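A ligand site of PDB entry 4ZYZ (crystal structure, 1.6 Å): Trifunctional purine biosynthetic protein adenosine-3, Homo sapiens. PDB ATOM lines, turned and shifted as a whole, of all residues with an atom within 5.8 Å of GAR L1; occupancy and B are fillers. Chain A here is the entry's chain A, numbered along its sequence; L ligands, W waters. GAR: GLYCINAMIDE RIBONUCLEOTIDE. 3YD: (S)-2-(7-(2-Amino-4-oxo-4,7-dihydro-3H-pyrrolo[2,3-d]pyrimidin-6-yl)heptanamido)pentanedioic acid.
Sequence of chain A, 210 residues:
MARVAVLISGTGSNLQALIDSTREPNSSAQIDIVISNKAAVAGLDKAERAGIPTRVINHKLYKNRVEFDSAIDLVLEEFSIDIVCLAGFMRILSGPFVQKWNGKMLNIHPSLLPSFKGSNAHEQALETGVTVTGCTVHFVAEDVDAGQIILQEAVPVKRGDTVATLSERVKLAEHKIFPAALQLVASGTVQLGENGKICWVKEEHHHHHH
Water W1 lies within hydrogen-bond range of an oxygen (O17) of GAR L1 (2.6 Å) and the backbone NH (N) of Thr 11 (2.9 Å).
Water W5 lies within hydrogen-bond range of an oxygen (O18) of GAR L1 (2.7 Å), the backbone NH (N) of Leu 15 (2.9 Å), the backbone carbonyl oxygen (O) of Ala 87 (2.9 Å) and the backbone NH (N) of Asn 14 (3.3 Å).
Water W9 lies within hydrogen-bond range of OD1 of Asp 145, N24 of GAR L1, ND1 of His 109 and ND2 of Asn 107.
Water W8 lies within hydrogen-bond range of O of Ile 108 (2.7 Å), N19 of GAR L1 (2.8 Å) and N of Gly 88 (2.9 Å).
Water W4 lies within hydrogen-bond range of O of Ala 87, O17 of GAR L1, N of Gly 10 and O of Gly 88.
Water W3 lies within hydrogen-bond range of OE2 of Glu 174 (2.6 Å), NE2 of His 122 (2.8 Å), O of Ser 167 (3.1 Å) and O6 of GAR L1 (3.3 Å).
The side-chain hydroxyl (OG) of Ser 13 is in hydrogen-bond range of a ring nitrogen (NE2) of His 175 (2.8 Å).
OE1 of Glu 174 is in hydrogen-bond range of ND2 of Asn 14 (2.7 Å).
A ring nitrogen (ND1) of His 175 lies close to the backbone carbonyl oxygen of Lys 171 (3.2 Å).
ND1 of His 109 sits close to OD2 of Asp 145.
The backbone NH (N) of Gly 118 sits at hydrogen-bond distance from the side-chain carboxylate (OD2) of Asp 145.
Residues that only touch GAR L1: Pro 110 (3.3 Å), Lys 171 (3.3 Å), Thr 11 (3.5 Å), Gly 88 (3.6 Å), Met 90 (3.7 Å), Ile 108 (3.8 Å), His 109 (3.8 Å) and Gly 118 (3.9 Å).
Hydrophobic or aromatic side chains that line GAR L1: Met 90, Ile 108 and Pro 110.
The nearest printed residue that does not touch GAR L1 is Gly 10 (4.2 Å).
The backbone NH of Ser 13 lies within hydrogen-bond range of an oxygen (O16) of GAR L1 (2.9 Å).
An oxygen (O16) of GAR L1 lies within hydrogen-bond range of the side-chain hydroxyl (OG) of Ser 13, 2.6 Å away.
An oxygen (O6) of GAR L1 lies within hydrogen-bond range of the side-chain carboxylate of Glu 174, 2.8 Å away.
The backbone NH of Gly 12 lies within hydrogen-bond range of an oxygen (O17) of GAR L1 (2.9 Å).
The backbone NH (N) of Asn 14 sits at hydrogen-bond distance from an oxygen (O18) of GAR L1 (3.0 Å).
The side-chain amide nitrogen of Asn 14 sits at hydrogen-bond distance from an oxygen (O18) of GAR L1 (3.1 Å).
An oxygen (O24) of 3YD L2 sits close to the backbone carbonyl oxygen of Met 90.
The backbone NH of Asp 145 sits at hydrogen-bond distance from an oxygen (O10) of 3YD L2 (3.0 Å).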
ATOM      1  N   GLY A  10      23.315   0.773   9.776  1.00  0.00           N
ATOM      2  CA  GLY A  10      23.750   1.969   9.068  1.00  0.00           C
ATOM      3  C   GLY A  10      25.144   2.015   8.466  1.00  0.00           C
ATOM      4  O   GLY A  10      25.563   1.096   7.760  1.00  0.00           O
ATOM      5  N   THR A  11      25.853   3.113   8.758  1.00  0.00           N
ATOM      6  CA  THR A  11      27.126   3.432   8.129  1.00  0.00           C
ATOM      7  C   THR A  11      28.193   2.352   8.313  1.00  0.00           C
ATOM      8  O   THR A  11      28.912   1.990   7.368  1.00  0.00           O
ATOM      9  CB  THR A  11      27.674   4.768   8.691  1.00  0.00           C
ATOM     10  OG1 THR A  11      26.745   5.817   8.389  1.00  0.00           O
ATOM     11  CG2 THR A  11      29.034   5.104   8.079  1.00  0.00           C
ATOM     12  N   GLY A  12      28.310   1.843   9.527  1.00  0.00           N
ATOM     13  CA  GLY A  12      29.226   0.758   9.803  1.00  0.00           C
ATOM     14  C   GLY A  12      30.659   1.131  10.123  1.00  0.00           C
ATOM     15  O   GLY A  12      31.567   0.322   9.914  1.00  0.00           O
ATOM     16  N   SER A  13      30.899   2.335  10.648  1.00  0.00           N
ATOM     17  CA  SER A  13      32.266   2.662  11.050  1.00  0.00           C
ATOM     18  C   SER A  13      32.721   1.780  12.203  1.00  0.00           C
ATOM     19  O   SER A  13      33.892   1.373  12.237  1.00  0.00           O
ATOM     20  CB  SER A  13      32.410   4.155  11.419  1.00  0.00           C
ATOM     21  OG  SER A  13      31.776   4.452  12.650  1.00  0.00           O
ATOM     22  N   ASN A  14      31.838   1.469  13.152  1.00  0.00           N
ATOM     23  CA  ASN A  14      32.231   0.543  14.215  1.00  0.00           C
ATOM     24  C   ASN A  14      32.509  -0.841  13.643  1.00  0.00           C
ATOM     25  O   ASN A  14      33.459  -1.496  14.064  1.00  0.00           O
ATOM     26  CB  ASN A  14      31.166   0.474  15.324  1.00  0.00           C
ATOM     27  CG  ASN A  14      31.352   1.570  16.368  1.00  0.00           C
ATOM     28  OD1 ASN A  14      32.282   1.532  17.159  1.00  0.00           O
ATOM     29  ND2 ASN A  14      30.444   2.536  16.375  1.00  0.00           N
ATOM     30  N   LEU A  15      31.683  -1.285  12.691  1.00  0.00           N
ATOM     31  CA  LEU A  15      31.931  -2.552  12.022  1.00  0.00           C
ATOM     32  C   LEU A  15      33.326  -2.572  11.397  1.00  0.00           C
ATOM     33  O   LEU A  15      34.055  -3.545  11.569  1.00  0.00           O
ATOM     34  CB  LEU A  15      30.872  -2.816  10.942  1.00  0.00           C
ATOM     35  CG  LEU A  15      31.198  -3.945   9.961  1.00  0.00           C
ATOM     36  CD1 LEU A  15      31.331  -5.305  10.659  1.00  0.00           C
ATOM     37  CD2 LEU A  15      30.126  -4.000   8.883  1.00  0.00           C
ATOM     38  N   ALA A  87      26.463  -3.014  16.575  1.00  0.00           N
ATOM     39  CA  ALA A  87      27.330  -1.917  16.151  1.00  0.00           C
ATOM     40  C   ALA A  87      26.520  -0.951  15.296  1.00  0.00           C
ATOM     41  O   ALA A  87      26.506  -1.025  14.074  1.00  0.00           O
ATOM     42  CB  ALA A  87      28.535  -2.458  15.381  1.00  0.00           C
ATOM     43  N   GLY A  88      25.829  -0.035  15.962  1.00  0.00           N
ATOM     44  CA  GLY A  88      24.906   0.854  15.272  1.00  0.00           C
ATOM     45  C   GLY A  88      23.599   0.181  14.913  1.00  0.00           C
ATOM     46  O   GLY A  88      22.830   0.694  14.102  1.00  0.00           O
ATOM     47  N   PHE A  89      23.340  -0.989  15.512  1.00  0.00           N
ATOM     48  CA  PHE A  89      22.071  -1.689  15.352  1.00  0.00           C
ATOM     49  C   PHE A  89      21.017  -1.001  16.199  1.00  0.00           C
ATOM     50  O   PHE A  89      21.195  -0.852  17.404  1.00  0.00           O
ATOM     51  CB  PHE A  89      22.244  -3.164  15.768  1.00  0.00           C
ATOM     52  CG  PHE A  89      21.016  -4.008  15.590  1.00  0.00           C
ATOM     53  CD1 PHE A  89      20.647  -4.462  14.327  1.00  0.00           C
ATOM     54  CD2 PHE A  89      20.249  -4.376  16.678  1.00  0.00           C
ATOM     55  CE1 PHE A  89      19.521  -5.256  14.158  1.00  0.00           C
ATOM     56  CE2 PHE A  89      19.129  -5.183  16.526  1.00  0.00           C
ATOM     57  CZ  PHE A  89      18.758  -5.614  15.264  1.00  0.00           C
ATOM     58  N   MET A  90      19.915  -0.565  15.589  1.00  0.00           N
ATOM     59  CA  MET A  90      19.021   0.339  16.306  1.00  0.00           C
ATOM     60  C   MET A  90      17.669  -0.286  16.638  1.00  0.00           C
ATOM     61  O   MET A  90      16.664   0.423  16.645  1.00  0.00           O
ATOM     62  CB  MET A  90      18.815   1.636  15.507  1.00  0.00           C
ATOM     63  CG  MET A  90      20.091   2.440  15.240  1.00  0.00           C
ATOM     64  SD  MET A  90      21.063   2.856  16.708  1.00  0.00           S
ATOM     65  CE  MET A  90      19.977   4.024  17.518  1.00  0.00           C
ATOM     66  N   ASN A 107      27.091  -4.283  23.187  1.00  0.00           N
ATOM     67  CA  ASN A 107      26.579  -3.105  22.480  1.00  0.00           C
ATOM     68  C   ASN A 107      27.488  -1.912  22.704  1.00  0.00           C
ATOM     69  O   ASN A 107      28.089  -1.783  23.769  1.00  0.00           O
ATOM     70  CB  ASN A 107      25.154  -2.772  22.969  1.00  0.00           C
ATOM     71  CG  ASN A 107      24.561  -1.558  22.285  1.00  0.00           C
ATOM     72  OD1 ASN A 107      24.430  -1.526  21.060  1.00  0.00           O
ATOM     73  ND2 ASN A 107      24.185  -0.547  23.074  1.00  0.00           N
ATOM     74  N   ILE A 108      27.567  -1.024  21.715  1.00  0.00           N
ATOM     75  CA  ILE A 108      28.275   0.255  21.884  1.00  0.00           C
ATOM     76  C   ILE A 108      27.227   1.357  21.968  1.00  0.00           C
ATOM     77  O   ILE A 108      26.264   1.390  21.209  1.00  0.00           O
ATOM     78  CB  ILE A 108      29.287   0.532  20.741  1.00  0.00           C
ATOM     79  CG1 ILE A 108      30.027   1.856  20.972  1.00  0.00           C
ATOM     80  CG2 ILE A 108      28.628   0.557  19.374  1.00  0.00           C
ATOM     81  CD1 ILE A 108      31.347   1.696  21.613  1.00  0.00           C
ATOM     82  N   HIS A 109      27.420   2.260  22.924  1.00  0.00           N
ATOM     83  CA  HIS A 109      26.481   3.354  23.136  1.00  0.00           C
ATOM     84  C   HIS A 109      27.279   4.650  23.299  1.00  0.00           C
ATOM     85  O   HIS A 109      28.233   4.679  24.053  1.00  0.00           O
ATOM     86  CB  HIS A 109      25.641   3.094  24.380  1.00  0.00           C
ATOM     87  CG  HIS A 109      24.665   4.172  24.677  1.00  0.00           C
ATOM     88  ND1 HIS A 109      23.425   4.253  24.068  1.00  0.00           N
ATOM     89  CD2 HIS A 109      24.736   5.230  25.515  1.00  0.00           C
ATOM     90  CE1 HIS A 109      22.783   5.318  24.514  1.00  0.00           C
ATOM     91  NE2 HIS A 109      23.553   5.922  25.399  1.00  0.00           N
ATOM     92  N   PRO A 110      26.863   5.717  22.593  1.00  0.00           N
ATOM     93  CA  PRO A 110      27.678   6.942  22.560  1.00  0.00           C
ATOM     94  C   PRO A 110      27.414   7.922  23.703  1.00  0.00           C
ATOM     95  O   PRO A 110      27.221   9.121  23.484  1.00  0.00           O
ATOM     96  CB  PRO A 110      27.292   7.565  21.213  1.00  0.00           C
ATOM     97  CG  PRO A 110      25.847   7.179  21.073  1.00  0.00           C
ATOM     98  CD  PRO A 110      25.743   5.778  21.649  1.00  0.00           C
ATOM     99  N   GLY A 118      19.318   5.730  25.696  1.00  0.00           N
ATOM    100  CA  GLY A 118      18.362   5.948  24.617  1.00  0.00           C
ATOM    101  C   GLY A 118      18.986   6.356  23.290  1.00  0.00           C
ATOM    102  O   GLY A 118      20.197   6.348  23.142  1.00  0.00           O
ATOM    103  N   SER A 119      18.138   6.768  22.342  1.00  0.00           N
ATOM    104  CA  SER A 119      18.539   6.807  20.928  1.00  0.00           C
ATOM    105  C   SER A 119      19.242   8.066  20.426  1.00  0.00           C
ATOM    106  O   SER A 119      19.881   8.047  19.363  1.00  0.00           O
ATOM    107  CB  SER A 119      17.296   6.587  20.071  1.00  0.00           C
ATOM    108  OG  SER A 119      16.424   7.675  20.260  1.00  0.00           O
ATOM    109  N   HIS A 122      23.720  12.114  21.925  1.00  0.00           N
ATOM    110  CA  HIS A 122      24.454  13.369  21.725  1.00  0.00           C
ATOM    111  C   HIS A 122      23.537  14.566  21.905  1.00  0.00           C
ATOM    112  O   HIS A 122      23.939  15.577  22.489  1.00  0.00           O
ATOM    113  CB  HIS A 122      25.103  13.426  20.350  1.00  0.00           C
ATOM    114  CG  HIS A 122      26.111  12.344  20.128  1.00  0.00           C
ATOM    115  ND1 HIS A 122      27.194  12.157  20.960  1.00  0.00           N
ATOM    116  CD2 HIS A 122      26.194  11.392  19.170  1.00  0.00           C
ATOM    117  CE1 HIS A 122      27.905  11.131  20.514  1.00  0.00           C
ATOM    118  NE2 HIS A 122      27.328  10.653  19.433  1.00  0.00           N
ATOM    119  N   ASP A 145      20.343  -0.334  27.596  1.00  0.00           N
ATOM    120  CA  ASP A 145      21.479   0.481  28.036  1.00  0.00           C
ATOM    121  C   ASP A 145      21.747   0.358  29.537  1.00  0.00           C
ATOM    122  O   ASP A 145      22.366   1.245  30.135  1.00  0.00           O
ATOM    123  CB  ASP A 145      21.269   1.956  27.639  1.00  0.00           C
ATOM    124  CG  ASP A 145      21.259   2.155  26.123  1.00  0.00           C
ATOM    125  OD1 ASP A 145      21.755   1.258  25.399  1.00  0.00           O
ATOM    126  OD2 ASP A 145      20.768   3.204  25.668  1.00  0.00           O
ATOM    127  N   SER A 167      29.500  13.716  17.561  1.00  0.00           N
ATOM    128  CA  SER A 167      29.433  12.302  17.204  1.00  0.00           C
ATOM    129  C   SER A 167      30.722  11.873  16.519  1.00  0.00           C
ATOM    130  O   SER A 167      31.229  10.772  16.746  1.00  0.00           O
ATOM    131  CB  SER A 167      28.220  12.006  16.310  1.00  0.00           C
ATOM    132  OG  SER A 167      28.325  12.647  15.050  1.00  0.00           O
ATOM    133  N   LYS A 171      33.039   8.938  17.968  1.00  0.00           N
ATOM    134  CA  LYS A 171      33.281   7.730  17.181  1.00  0.00           C
ATOM    135  C   LYS A 171      34.743   7.318  17.177  1.00  0.00           C
ATOM    136  O   LYS A 171      35.034   6.126  17.109  1.00  0.00           O
ATOM    137  CB  LYS A 171      32.780   7.927  15.740  1.00  0.00           C
ATOM    138  CG  LYS A 171      31.280   7.695  15.649  1.00  0.00           C
ATOM    139  CD  LYS A 171      30.781   7.644  14.227  1.00  0.00           C
ATOM    140  CE  LYS A 171      29.305   7.292  14.179  1.00  0.00           C
ATOM    141  NZ  LYS A 171      28.435   8.465  14.406  1.00  0.00           N
ATOM    142  N   GLU A 174      34.904   5.250  20.126  1.00  0.00           N
ATOM    143  CA  GLU A 174      34.123   4.024  19.936  1.00  0.00           C
ATOM    144  C   GLU A 174      34.980   2.991  19.223  1.00  0.00           C
ATOM    145  O   GLU A 174      34.970   1.806  19.582  1.00  0.00           O
ATOM    146  CB  GLU A 174      32.858   4.286  19.119  1.00  0.00           C
ATOM    147  CG  GLU A 174      31.852   5.197  19.811  1.00  0.00           C
ATOM    148  CD  GLU A 174      30.606   5.398  18.997  1.00  0.00           C
ATOM    149  OE1 GLU A 174      30.190   4.439  18.311  1.00  0.00           O
ATOM    150  OE2 GLU A 174      30.041   6.505  19.018  1.00  0.00           O
ATOM    151  N   HIS A 175      35.729   3.448  18.220  1.00  0.00           N
ATOM    152  CA  HIS A 175      36.551   2.560  17.398  1.00  0.00           C
ATOM    153  C   HIS A 175      37.746   1.992  18.142  1.00  0.00           C
ATOM    154  O   HIS A 175      38.412   1.084  17.659  1.00  0.00           O
ATOM    155  CB  HIS A 175      37.017   3.295  16.161  1.00  0.00           C
ATOM    156  CG  HIS A 175      35.895   3.788  15.312  1.00  0.00           C
ATOM    157  ND1 HIS A 175      36.058   4.769  14.361  1.00  0.00           N
ATOM    158  CD2 HIS A 175      34.593   3.443  15.290  1.00  0.00           C
ATOM    159  CE1 HIS A 175      34.894   5.005  13.784  1.00  0.00           C
ATOM    160  NE2 HIS A 175      33.982   4.217  14.327  1.00  0.00           N
HETATM  161  C1  GAR L   1      27.548   4.900  16.845  1.00  0.00           C
HETATM  162  O6  GAR L   1      27.884   6.211  17.308  1.00  0.00           O
HETATM  163  C2  GAR L   1      26.933   4.119  17.979  1.00  0.00           C
HETATM  164  O8  GAR L   1      27.550   4.345  19.255  1.00  0.00           O
HETATM  165  C3  GAR L   1      25.483   4.605  17.944  1.00  0.00           C
HETATM  166  O4  GAR L   1      25.210   4.665  16.554  1.00  0.00           O
HETATM  167  C5  GAR L   1      26.405   4.993  15.834  1.00  0.00           C
HETATM  168  C10 GAR L   1      26.615   3.998  14.711  1.00  0.00           C
HETATM  169  O12 GAR L   1      27.685   4.399  13.869  1.00  0.00           O
HETATM  170  N19 GAR L   1      24.615   3.691  18.630  1.00  0.00           N
HETATM  171  C21 GAR L   1      23.575   4.111  19.344  1.00  0.00           C
HETATM  172  O22 GAR L   1      23.215   5.284  19.380  1.00  0.00           O
HETATM  173  C23 GAR L   1      22.829   3.035  20.107  1.00  0.00           C
HETATM  174  N24 GAR L   1      21.659   3.552  20.802  1.00  0.00           N
HETATM  175  P15 GAR L   1      28.353   3.371  12.810  1.00  0.00           P
HETATM  176  O16 GAR L   1      29.294   4.251  12.033  1.00  0.00           O
HETATM  177  O17 GAR L   1      27.176   2.817  12.022  1.00  0.00           O
HETATM  178  O18 GAR L   1      29.026   2.328  13.664  1.00  0.00           O
HETATM  179  N1  3YD L   2      17.912  -4.341  23.344  1.00  0.00           N
HETATM  180  C2  3YD L   2      17.885  -4.623  24.693  1.00  0.00           C
HETATM  181  N3  3YD L   2      18.891  -4.117  25.563  1.00  0.00           N
HETATM  182  C4  3YD L   2      19.877  -3.258  25.094  1.00  0.00           C
HETATM  183  N5  3YD L   2      19.233  -3.032  21.693  1.00  0.00           N
HETATM  184  C6  3YD L   2      20.231  -2.293  21.678  1.00  0.00           C
HETATM  185  C7  3YD L   2      20.710  -2.199  22.855  1.00  0.00           C
HETATM  186  C8  3YD L   2      19.929  -2.961  23.766  1.00  0.00           C
HETATM  187  C9  3YD L   2      18.870  -3.544  22.900  1.00  0.00           C
HETATM  188  O10 3YD L   2      20.672  -2.843  25.919  1.00  0.00           O
HETATM  189  N11 3YD L   2      16.876  -5.479  25.233  1.00  0.00           N
HETATM  190  C12 3YD L   2      15.860   1.266  19.531  1.00  0.00           C
HETATM  191  C13 3YD L   2      17.049   1.759  20.379  1.00  0.00           C
HETATM  192  C14 3YD L   2      18.405   1.283  19.805  1.00  0.00           C
HETATM  193  C15 3YD L   2      18.864   0.001  20.506  1.00  0.00           C
HETATM  194  C16 3YD L   2      20.399  -0.126  20.425  1.00  0.00           C
HETATM  195  C17 3YD L   2      14.676   2.247  19.717  1.00  0.00           C
HETATM  196  O18 3YD L   2      14.852   3.179  20.469  1.00  0.00           O
HETATM  197  N19 3YD L   2      13.381   2.162  19.066  1.00  0.00           N
HETATM  198  C20 3YD L   2      12.866   1.177  18.119  1.00  0.00           C
HETATM  199  C21 3YD L   2      13.740   1.025  16.911  1.00  0.00           C
HETATM  200  C22 3YD L   2      13.545   2.135  15.884  1.00  0.00           C
HETATM  201  C23 3YD L   2      14.603   1.986  14.816  1.00  0.00           C
HETATM  202  O24 3YD L   2      15.674   2.657  14.887  1.00  0.00           O
HETATM  203  O25 3YD L   2      14.430   1.189  13.861  1.00  0.00           O
HETATM  204  C26 3YD L   2      12.648  -0.166  18.760  1.00  0.00           C
HETATM  205  O27 3YD L   2      11.684  -0.343  19.547  1.00  0.00           O
HETATM  206  O28 3YD L   2      13.400  -1.142  18.485  1.00  0.00           O
HETATM  207  C29 3YD L   2      20.825  -1.599  20.433  1.00  0.00           C
HETATM  208  O   HOH W   1      25.153   4.338  11.342  1.00  0.00           O
HETATM  209  O   HOH W   2      29.247   6.906  11.110  1.00  0.00           O
HETATM  210  O   HOH W   3      29.342   8.980  18.384  1.00  0.00           O
HETATM  211  O   HOH W   4      25.503   0.480  11.860  1.00  0.00           O
HETATM  212  O   HOH W   5      28.989  -0.208  12.774  1.00  0.00           O
HETATM  213  O   HOH W   6      22.234   7.332  21.267  1.00  0.00           O
HETATM  214  O   HOH W   7      26.527   8.531  17.098  1.00  0.00           O
HETATM  215  O   HOH W   8      25.401   0.956  18.681  1.00  0.00           O
HETATM  216  O   HOH W   9      22.403   1.922  22.896  1.00  0.00           O
